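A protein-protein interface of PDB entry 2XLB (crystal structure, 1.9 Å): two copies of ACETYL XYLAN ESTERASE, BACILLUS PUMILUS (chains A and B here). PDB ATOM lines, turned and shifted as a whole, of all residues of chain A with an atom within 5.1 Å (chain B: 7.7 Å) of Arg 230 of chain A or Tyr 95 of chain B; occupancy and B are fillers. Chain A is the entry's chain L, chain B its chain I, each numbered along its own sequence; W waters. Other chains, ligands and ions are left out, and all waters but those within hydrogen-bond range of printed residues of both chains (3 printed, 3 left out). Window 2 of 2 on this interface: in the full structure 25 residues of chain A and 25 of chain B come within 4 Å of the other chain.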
ATOM      1  N   ASN A 226      19.636  16.007  11.129  1.00  0.00           N
ATOM      2  CA  ASN A 226      20.412  15.438  10.039  1.00  0.00           C
ATOM      3  C   ASN A 226      21.201  14.224  10.544  1.00  0.00           C
ATOM      4  O   ASN A 226      21.197  13.168   9.910  1.00  0.00           O
ATOM      5  CB  ASN A 226      21.372  16.471   9.432  1.00  0.00           C
ATOM      6  CG  ASN A 226      20.664  17.769   8.996  1.00  0.00           C
ATOM      7  OD1 ASN A 226      19.880  18.352   9.747  1.00  0.00           O
ATOM      8  ND2 ASN A 226      20.955  18.222   7.786  1.00  0.00           N
ATOM      9  N   SER A 227      21.864  14.390  11.690  1.00  0.00           N
ATOM     10  CA  SER A 227      22.622  13.312  12.329  1.00  0.00           C
ATOM     11  C   SER A 227      21.756  12.079  12.561  1.00  0.00           C
ATOM     12  O   SER A 227      22.180  10.949  12.323  1.00  0.00           O
ATOM     13  CB  SER A 227      23.195  13.799  13.668  1.00  0.00           C
ATOM     14  OG  SER A 227      24.388  14.510  13.449  1.00  0.00           O
ATOM     15  N   TYR A 228      20.536  12.324  13.021  1.00  0.00           N
ATOM     16  CA  TYR A 228      19.587  11.256  13.309  1.00  0.00           C
ATOM     17  C   TYR A 228      19.240  10.471  12.033  1.00  0.00           C
ATOM     18  O   TYR A 228      19.206   9.248  12.035  1.00  0.00           O
ATOM     19  CB  TYR A 228      18.330  11.848  13.955  1.00  0.00           C
ATOM     20  CG  TYR A 228      17.246  10.832  14.230  1.00  0.00           C
ATOM     21  CD1 TYR A 228      16.154  10.708  13.389  1.00  0.00           C
ATOM     22  CD2 TYR A 228      17.341   9.968  15.304  1.00  0.00           C
ATOM     23  CE1 TYR A 228      15.162   9.771  13.632  1.00  0.00           C
ATOM     24  CE2 TYR A 228      16.358   9.020  15.552  1.00  0.00           C
ATOM     25  CZ  TYR A 228      15.266   8.932  14.711  1.00  0.00           C
ATOM     26  OH  TYR A 228      14.282   7.992  14.953  1.00  0.00           O
ATOM     27  N   PHE A 229      19.001  11.187  10.935  1.00  0.00           N
ATOM     28  CA  PHE A 229      18.674  10.530   9.665  1.00  0.00           C
ATOM     29  C   PHE A 229      19.862   9.773   9.072  1.00  0.00           C
ATOM     30  O   PHE A 229      19.672   8.799   8.353  1.00  0.00           O
ATOM     31  CB  PHE A 229      18.135  11.527   8.644  1.00  0.00           C
ATOM     32  CG  PHE A 229      16.851  12.203   9.060  1.00  0.00           C
ATOM     33  CD1 PHE A 229      16.608  13.506   8.682  1.00  0.00           C
ATOM     34  CD2 PHE A 229      15.903  11.546   9.838  1.00  0.00           C
ATOM     35  CE1 PHE A 229      15.441  14.153   9.048  1.00  0.00           C
ATOM     36  CE2 PHE A 229      14.728  12.189  10.217  1.00  0.00           C
ATOM     37  CZ  PHE A 229      14.502  13.497   9.815  1.00  0.00           C
ATOM     38  N   ARG A 230      21.053  10.211   9.372  1.00  0.00           N
ATOM     39  CA  ARG A 230      22.221   9.516   8.923  1.00  0.00           C
ATOM     40  C   ARG A 230      22.263   8.112   9.590  1.00  0.00           C
ATOM     41  O   ARG A 230      22.596   7.166   8.924  1.00  0.00           O
ATOM     42  CB  ARG A 230      23.494  10.313   9.164  1.00  0.00           C
ATOM     43  CG  ARG A 230      23.581  11.577   8.379  1.00  0.00           C
ATOM     44  CD  ARG A 230      24.739  12.395   8.687  1.00  0.00           C
ATOM     45  NE  ARG A 230      25.914  11.687   8.930  1.00  0.00           N
ATOM     46  CZ  ARG A 230      26.865  11.454   8.040  1.00  0.00           C
ATOM     47  NH1 ARG A 230      26.787  11.924   6.844  1.00  0.00           N
ATOM     48  NH2 ARG A 230      27.901  10.789   8.390  1.00  0.00           N
ATOM     49  N   ARG A 231      21.924   8.076  10.872  1.00  0.00           N
ATOM     50  CA  ARG A 231      21.987   6.869  11.691  1.00  0.00           C
ATOM     51  C   ARG A 231      20.785   5.941  11.495  1.00  0.00           C
ATOM     52  O   ARG A 231      20.878   4.740  11.711  1.00  0.00           O
ATOM     53  CB  ARG A 231      22.141   7.254  13.161  1.00  0.00           C
ATOM     54  CG  ARG A 231      23.515   7.777  13.477  1.00  0.00           C
ATOM     55  CD  ARG A 231      23.531   8.671  14.704  1.00  0.00           C
ATOM     56  NE  ARG A 231      24.900   9.053  15.028  1.00  0.00           N
ATOM     57  CZ  ARG A 231      25.626   9.932  14.345  1.00  0.00           C
ATOM     58  NH1 ARG A 231      25.119  10.551  13.288  1.00  0.00           N
ATOM     59  NH2 ARG A 231      26.871  10.191  14.718  1.00  0.00           N
ATOM     60  N   ASN A 232      19.672   6.505  11.051  1.00  0.00           N
ATOM     61  CA  ASN A 232      18.432   5.762  10.880  1.00  0.00           C
ATOM     62  C   ASN A 232      17.859   6.087   9.502  1.00  0.00           C
ATOM     63  O   ASN A 232      17.119   7.045   9.325  1.00  0.00           O
ATOM     64  CB  ASN A 232      17.477   6.146  12.005  1.00  0.00           C
ATOM     65  CG  ASN A 232      18.109   5.959  13.388  1.00  0.00           C
ATOM     66  OD1 ASN A 232      18.131   4.854  13.924  1.00  0.00           O
ATOM     67  ND2 ASN A 232      18.661   7.033  13.942  1.00  0.00           N
ATOM     68  N   SER A 233      18.240   5.285   8.517  1.00  0.00           N
ATOM     69  CA  SER A 233      18.082   5.654   7.109  1.00  0.00           C
ATOM     70  C   SER A 233      16.753   5.259   6.463  1.00  0.00           C
ATOM     71  O   SER A 233      16.521   5.587   5.299  1.00  0.00           O
ATOM     72  CB  SER A 233      19.216   5.048   6.283  1.00  0.00           C
ATOM     73  OG  SER A 233      19.084   3.641   6.165  1.00  0.00           O
ATOM     74  N   PHE B  72      20.265  -6.575  15.967  1.00  0.00           N
ATOM     75  CA  PHE B  72      20.237  -7.665  15.009  1.00  0.00           C
ATOM     76  C   PHE B  72      21.073  -8.844  15.502  1.00  0.00           C
ATOM     77  O   PHE B  72      22.106  -8.677  16.140  1.00  0.00           O
ATOM     78  CB  PHE B  72      20.705  -7.190  13.625  1.00  0.00           C
ATOM     79  CG  PHE B  72      19.704  -6.324  12.930  1.00  0.00           C
ATOM     80  CD1 PHE B  72      19.987  -4.990  12.642  1.00  0.00           C
ATOM     81  CD2 PHE B  72      18.457  -6.836  12.575  1.00  0.00           C
ATOM     82  CE1 PHE B  72      19.049  -4.185  12.003  1.00  0.00           C
ATOM     83  CE2 PHE B  72      17.503  -6.027  11.938  1.00  0.00           C
ATOM     84  CZ  PHE B  72      17.807  -4.710  11.641  1.00  0.00           C
ATOM     85  N   ARG B  87      28.576  -8.083  20.092  1.00  0.00           N
ATOM     86  CA  ARG B  87      29.336  -6.961  19.574  1.00  0.00           C
ATOM     87  C   ARG B  87      28.708  -5.674  20.079  1.00  0.00           C
ATOM     88  O   ARG B  87      27.497  -5.512  19.969  1.00  0.00           O
ATOM     89  CB  ARG B  87      29.278  -6.977  18.048  1.00  0.00           C
ATOM     90  CG  ARG B  87      30.007  -5.815  17.390  1.00  0.00           C
ATOM     91  CD  ARG B  87      29.442  -5.566  16.023  1.00  0.00           C
ATOM     92  NE  ARG B  87      30.194  -4.517  15.330  1.00  0.00           N
ATOM     93  CZ  ARG B  87      29.731  -3.305  15.033  1.00  0.00           C
ATOM     94  NH1 ARG B  87      28.481  -2.936  15.333  1.00  0.00           N
ATOM     95  NH2 ARG B  87      30.528  -2.453  14.397  1.00  0.00           N
ATOM     96  N   HIS B  89      28.646  -1.421  20.026  1.00  0.00           N
ATOM     97  CA  HIS B  89      29.004  -0.325  19.125  1.00  0.00           C
ATOM     98  C   HIS B  89      29.592   0.879  19.848  1.00  0.00           C
ATOM     99  O   HIS B  89      29.477   1.002  21.053  1.00  0.00           O
ATOM    100  CB  HIS B  89      27.803   0.087  18.258  1.00  0.00           C
ATOM    101  CG  HIS B  89      26.661   0.696  19.015  1.00  0.00           C
ATOM    102  ND1 HIS B  89      26.696   1.987  19.503  1.00  0.00           N
ATOM    103  CD2 HIS B  89      25.431   0.216  19.305  1.00  0.00           C
ATOM    104  CE1 HIS B  89      25.542   2.263  20.084  1.00  0.00           C
ATOM    105  NE2 HIS B  89      24.755   1.208  19.977  1.00  0.00           N
ATOM    106  N   GLY B  90      30.217   1.760  19.078  1.00  0.00           N
ATOM    107  CA  GLY B  90      30.837   2.967  19.617  1.00  0.00           C
ATOM    108  C   GLY B  90      29.829   4.021  20.044  1.00  0.00           C
ATOM    109  O   GLY B  90      28.625   3.941  19.734  1.00  0.00           O
ATOM    110  N   TYR B  91      30.336   5.020  20.756  1.00  0.00           N
ATOM    111  CA  TYR B  91      29.512   6.098  21.307  1.00  0.00           C
ATOM    112  C   TYR B  91      28.903   6.910  20.168  1.00  0.00           C
ATOM    113  O   TYR B  91      29.628   7.461  19.341  1.00  0.00           O
ATOM    114  CB  TYR B  91      30.386   6.998  22.175  1.00  0.00           C
ATOM    115  CG  TYR B  91      29.650   8.047  22.958  1.00  0.00           C
ATOM    116  CD1 TYR B  91      29.112   7.758  24.204  1.00  0.00           C
ATOM    117  CD2 TYR B  91      29.561   9.346  22.493  1.00  0.00           C
ATOM    118  CE1 TYR B  91      28.479   8.716  24.940  1.00  0.00           C
ATOM    119  CE2 TYR B  91      28.905  10.313  23.216  1.00  0.00           C
ATOM    120  CZ  TYR B  91      28.372   9.997  24.440  1.00  0.00           C
ATOM    121  OH  TYR B  91      27.740  10.938  25.189  1.00  0.00           O
ATOM    122  N   ASN B  92      27.571   6.968  20.116  1.00  0.00           N
ATOM    123  CA  ASN B  92      26.867   7.717  19.085  1.00  0.00           C
ATOM    124  C   ASN B  92      27.290   7.305  17.671  1.00  0.00           C
ATOM    125  O   ASN B  92      27.231   8.106  16.746  1.00  0.00           O
ATOM    126  CB  ASN B  92      27.112   9.212  19.286  1.00  0.00           C
ATOM    127  CG  ASN B  92      26.203  10.082  18.438  1.00  0.00           C
ATOM    128  OD1 ASN B  92      24.998   9.838  18.335  1.00  0.00           O
ATOM    129  ND2 ASN B  92      26.776  11.111  17.839  1.00  0.00           N
ATOM    130  N   ALA B  93      27.704   6.054  17.518  1.00  0.00           N
ATOM    131  CA  ALA B  93      28.330   5.592  16.290  1.00  0.00           C
ATOM    132  C   ALA B  93      27.627   4.370  15.702  1.00  0.00           C
ATOM    133  O   ALA B  93      28.264   3.595  14.985  1.00  0.00           O
ATOM    134  CB  ALA B  93      29.802   5.281  16.536  1.00  0.00           C
ATOM    135  N   SER B  94      26.337   4.208  15.994  1.00  0.00           N
ATOM    136  CA  SER B  94      25.528   3.138  15.415  1.00  0.00           C
ATOM    137  C   SER B  94      24.721   3.646  14.223  1.00  0.00           C
ATOM    138  O   SER B  94      23.838   4.487  14.388  1.00  0.00           O
ATOM    139  CB  SER B  94      24.578   2.552  16.454  1.00  0.00           C
ATOM    140  OG  SER B  94      23.786   1.507  15.866  1.00  0.00           O
ATOM    141  N   TYR B  95      25.056   3.150  13.025  1.00  0.00           N
ATOM    142  CA  TYR B  95      24.356   3.520  11.791  1.00  0.00           C
ATOM    143  C   TYR B  95      23.588   2.313  11.287  1.00  0.00           C
ATOM    144  O   TYR B  95      24.177   1.264  11.012  1.00  0.00           O
ATOM    145  CB  TYR B  95      25.332   3.985  10.706  1.00  0.00           C
ATOM    146  CG  TYR B  95      26.036   5.293  11.023  1.00  0.00           C
ATOM    147  CD1 TYR B  95      27.028   5.346  11.982  1.00  0.00           C
ATOM    148  CD2 TYR B  95      25.702   6.467  10.365  1.00  0.00           C
ATOM    149  CE1 TYR B  95      27.667   6.540  12.294  1.00  0.00           C
ATOM    150  CE2 TYR B  95      26.338   7.671  10.665  1.00  0.00           C
ATOM    151  CZ  TYR B  95      27.316   7.691  11.639  1.00  0.00           C
ATOM    152  OH  TYR B  95      27.961   8.862  11.940  1.00  0.00           O
ATOM    153  N   ASP B  96      22.272   2.473  11.137  1.00  0.00           N
ATOM    154  CA  ASP B  96      21.393   1.370  10.735  1.00  0.00           C
ATOM    155  C   ASP B  96      21.689   0.092  11.536  1.00  0.00           C
ATOM    156  O   ASP B  96      21.728  -1.019  11.002  1.00  0.00           O
ATOM    157  CB  ASP B  96      21.476   1.156   9.224  1.00  0.00           C
ATOM    158  CG  ASP B  96      20.795   2.281   8.428  1.00  0.00           C
ATOM    159  OD1 ASP B  96      20.019   3.088   9.003  1.00  0.00           O
ATOM    160  OD2 ASP B  96      21.048   2.360   7.211  1.00  0.00           O
ATOM    161  N   ASP B  97      21.913   0.283  12.834  1.00  0.00           N
ATOM    162  CA  ASP B  97      22.070  -0.795  13.801  1.00  0.00           C
ATOM    163  C   ASP B  97      23.262  -1.724  13.517  1.00  0.00           C
ATOM    164  O   ASP B  97      23.290  -2.845  13.987  1.00  0.00           O
ATOM    165  CB  ASP B  97      20.762  -1.604  13.909  1.00  0.00           C
ATOM    166  CG  ASP B  97      19.537  -0.735  14.241  1.00  0.00           C
ATOM    167  OD1 ASP B  97      19.702   0.427  14.685  1.00  0.00           O
ATOM    168  OD2 ASP B  97      18.398  -1.230  14.060  1.00  0.00           O
ATOM    169  N   GLY B  98      24.255  -1.245  12.768  1.00  0.00           N
ATOM    170  CA  GLY B  98      25.451  -2.041  12.450  1.00  0.00           C
ATOM    171  C   GLY B  98      25.176  -3.330  11.688  1.00  0.00           C
ATOM    172  O   GLY B  98      25.963  -4.268  11.735  1.00  0.00           O
ATOM    173  N   ILE B  99      24.083  -3.384  10.948  1.00  0.00           N
ATOM    174  CA  ILE B  99      23.638  -4.652  10.365  1.00  0.00           C
ATOM    175  C   ILE B  99      24.681  -5.318   9.451  1.00  0.00           C
ATOM    176  O   ILE B  99      24.848  -6.530   9.482  1.00  0.00           O
ATOM    177  CB  ILE B  99      22.271  -4.508   9.629  1.00  0.00           C
ATOM    178  CG1 ILE B  99      21.750  -5.887   9.212  1.00  0.00           C
ATOM    179  CG2 ILE B  99      22.380  -3.557   8.439  1.00  0.00           C
ATOM    180  CD1 ILE B  99      20.287  -5.879   8.819  1.00  0.00           C
ATOM    181  N   HIS B 100      25.393  -4.524   8.664  1.00  0.00           N
ATOM    182  CA  HIS B 100      26.334  -5.063   7.688  1.00  0.00           C
ATOM    183  C   HIS B 100      27.511  -5.739   8.373  1.00  0.00           C
ATOM    184  O   HIS B 100      27.906  -6.835   7.959  1.00  0.00           O
ATOM    185  CB  HIS B 100      26.808  -3.974   6.722  1.00  0.00           C
ATOM    186  CG  HIS B 100      25.679  -3.213   6.095  1.00  0.00           C
ATOM    187  ND1 HIS B 100      24.755  -3.807   5.262  1.00  0.00           N
ATOM    188  CD2 HIS B 100      25.288  -1.924   6.230  1.00  0.00           C
ATOM    189  CE1 HIS B 100      23.859  -2.912   4.893  1.00  0.00           C
ATOM    190  NE2 HIS B 100      24.165  -1.757   5.458  1.00  0.00           N
ATOM    191  N   ASP B 101      28.031  -5.116   9.433  1.00  0.00           N
ATOM    192  CA  ASP B 101      29.089  -5.711  10.257  1.00  0.00           C
ATOM    193  C   ASP B 101      28.639  -7.004  10.928  1.00  0.00           C
ATOM    194  O   ASP B 101      29.403  -7.982  10.995  1.00  0.00           O
ATOM    195  CB  ASP B 101      29.543  -4.741  11.364  1.00  0.00           C
ATOM    196  CG  ASP B 101      30.611  -3.770  10.899  1.00  0.00           C
ATOM    197  OD1 ASP B 101      31.747  -3.837  11.416  1.00  0.00           O
ATOM    198  OD2 ASP B 101      30.316  -2.931  10.037  1.00  0.00           O
ATOM    199  N   LEU B 116      22.176  -2.906  20.797  1.00  0.00           N
ATOM    200  CA  LEU B 116      22.031  -1.462  20.615  1.00  0.00           C
ATOM    201  C   LEU B 116      22.003  -0.799  22.009  1.00  0.00           C
ATOM    202  O   LEU B 116      21.281  -1.222  22.907  1.00  0.00           O
ATOM    203  CB  LEU B 116      20.786  -1.162  19.782  1.00  0.00           C
ATOM    204  CG  LEU B 116      20.815  -1.788  18.374  1.00  0.00           C
ATOM    205  CD1 LEU B 116      19.486  -1.622  17.643  1.00  0.00           C
ATOM    206  CD2 LEU B 116      21.942  -1.185  17.550  1.00  0.00           C
ATOM    207  N   GLY B 121      21.797   3.725  19.699  1.00  0.00           N
ATOM    208  CA  GLY B 121      21.526   2.985  18.486  1.00  0.00           C
ATOM    209  C   GLY B 121      20.118   2.489  18.239  1.00  0.00           C
ATOM    210  O   GLY B 121      19.746   2.334  17.082  1.00  0.00           O
HETATM  211  O   HOH W   1      25.637  13.115  16.330  1.00  0.00           O
HETATM  212  O   HOH W   2      21.477   2.482  14.167  1.00  0.00           O
HETATM  213  O   HOH W   3      22.371   4.874   7.463  1.00  0.00           O
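Water W2 lies within hydrogen-bond range of the backbone NH (N) of Asp 97 of chain B (2.6 Å), the side-chain hydroxyl (OG) of Ser 94 of chain B (3.0 Å), the backbone NH (N) of Asp 96 of chain B (3.1 Å), the backbone carbonyl oxygen (O) of Arg 231 of chain A (3.4 Å) and the backbone carbonyl oxygen (O) of Gly 121 of chain B (3.4 Å). Water W3 lies within hydrogen-bond range of the backbone carbonyl oxygen of Arg 230 of chain A (2.7 Å) and the side-chain carboxylate of Asp 96 of chain B (2.9 Å). Water W1 bridges ND2 of Asn 92 of chain B (2.8 Å) and OG of Ser 227 of chain A (3.4 Å).
The guanidinium group of Arg 231 of chain A lies within hydrogen-bond range of the backbone carbonyl oxygen of Ser 227 of chain A, 3.1 Å away. The backbone carbonyl oxygen of Tyr 228 of chain A sits at hydrogen-bond distance from the side-chain amide nitrogen of Asn 232 of chain A, 3.0 Å away.
No position is printed for both chains. Of the 7 pairs that touch across the chains among the printed residues, none has its exchanged pair printed and touching as well.
Arg 230 of chain A touches just one residue of chain B: Tyr 95. Printed residues of chain B within 4 Å of Asn 232 of chain A: Asp 96. Of the printed residues of chain A, Asp 96 of chain B touches Arg 231, Asn 232 and Ser 233. Printed residues of chain A within 4 Å of Asn 92 of chain B: Arg 231 (2.9 Å). Printed residues of chain B within 4 Å of Ser 233 of chain A: Asp 96. The nearest residue of chain B that does not touch Arg 230 of chain A is Asp 96 of chain B (4.8 Å). The nearest printed residue of chain A that does not touch Asp 96 of chain B is Arg 230 of chain A (4.8 Å).
Among the printed residues, merely in contact across the chains: Arg 231 of chain A with Ser 94 of chain B, Arg 230 of chain A with Tyr 95 of chain B and Asn 232 of chain A with Asp 96 of chain B.
O of Asn 92 of chain B sits at hydrogen-bond distance from NH2 of Arg 231 of chain A, 2.9 Å away. NH2 of Arg 231 of chain A sits at hydrogen-bond distance from OH of Tyr 95 of chain B, at 3.3 Å. O of Arg 231 of chain A lies within hydrogen-bond range of N of Asp 96 of chain B (2.7 Å). The side-chain carboxylate of Asp 96 of chain B lies within hydrogen-bond range of the side-chain hydroxyl of Ser 233 of chain A (2.6 Å).
Of the 17 printed residues of chain B, 4 touch a printed residue of chain A. Hydrophobic or aromatic side chains of chain B within 4 Å of the printed part of chain A: Tyr 95. Printed residues of chain A that touch a printed residue of chain B: Arg 230, Arg 231, Asn 232 and Ser 233. Among the printed residues, no Asp or Glu carboxylate lies within 4 Å of a Lys or Arg side-chain nitrogen of the other chain.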
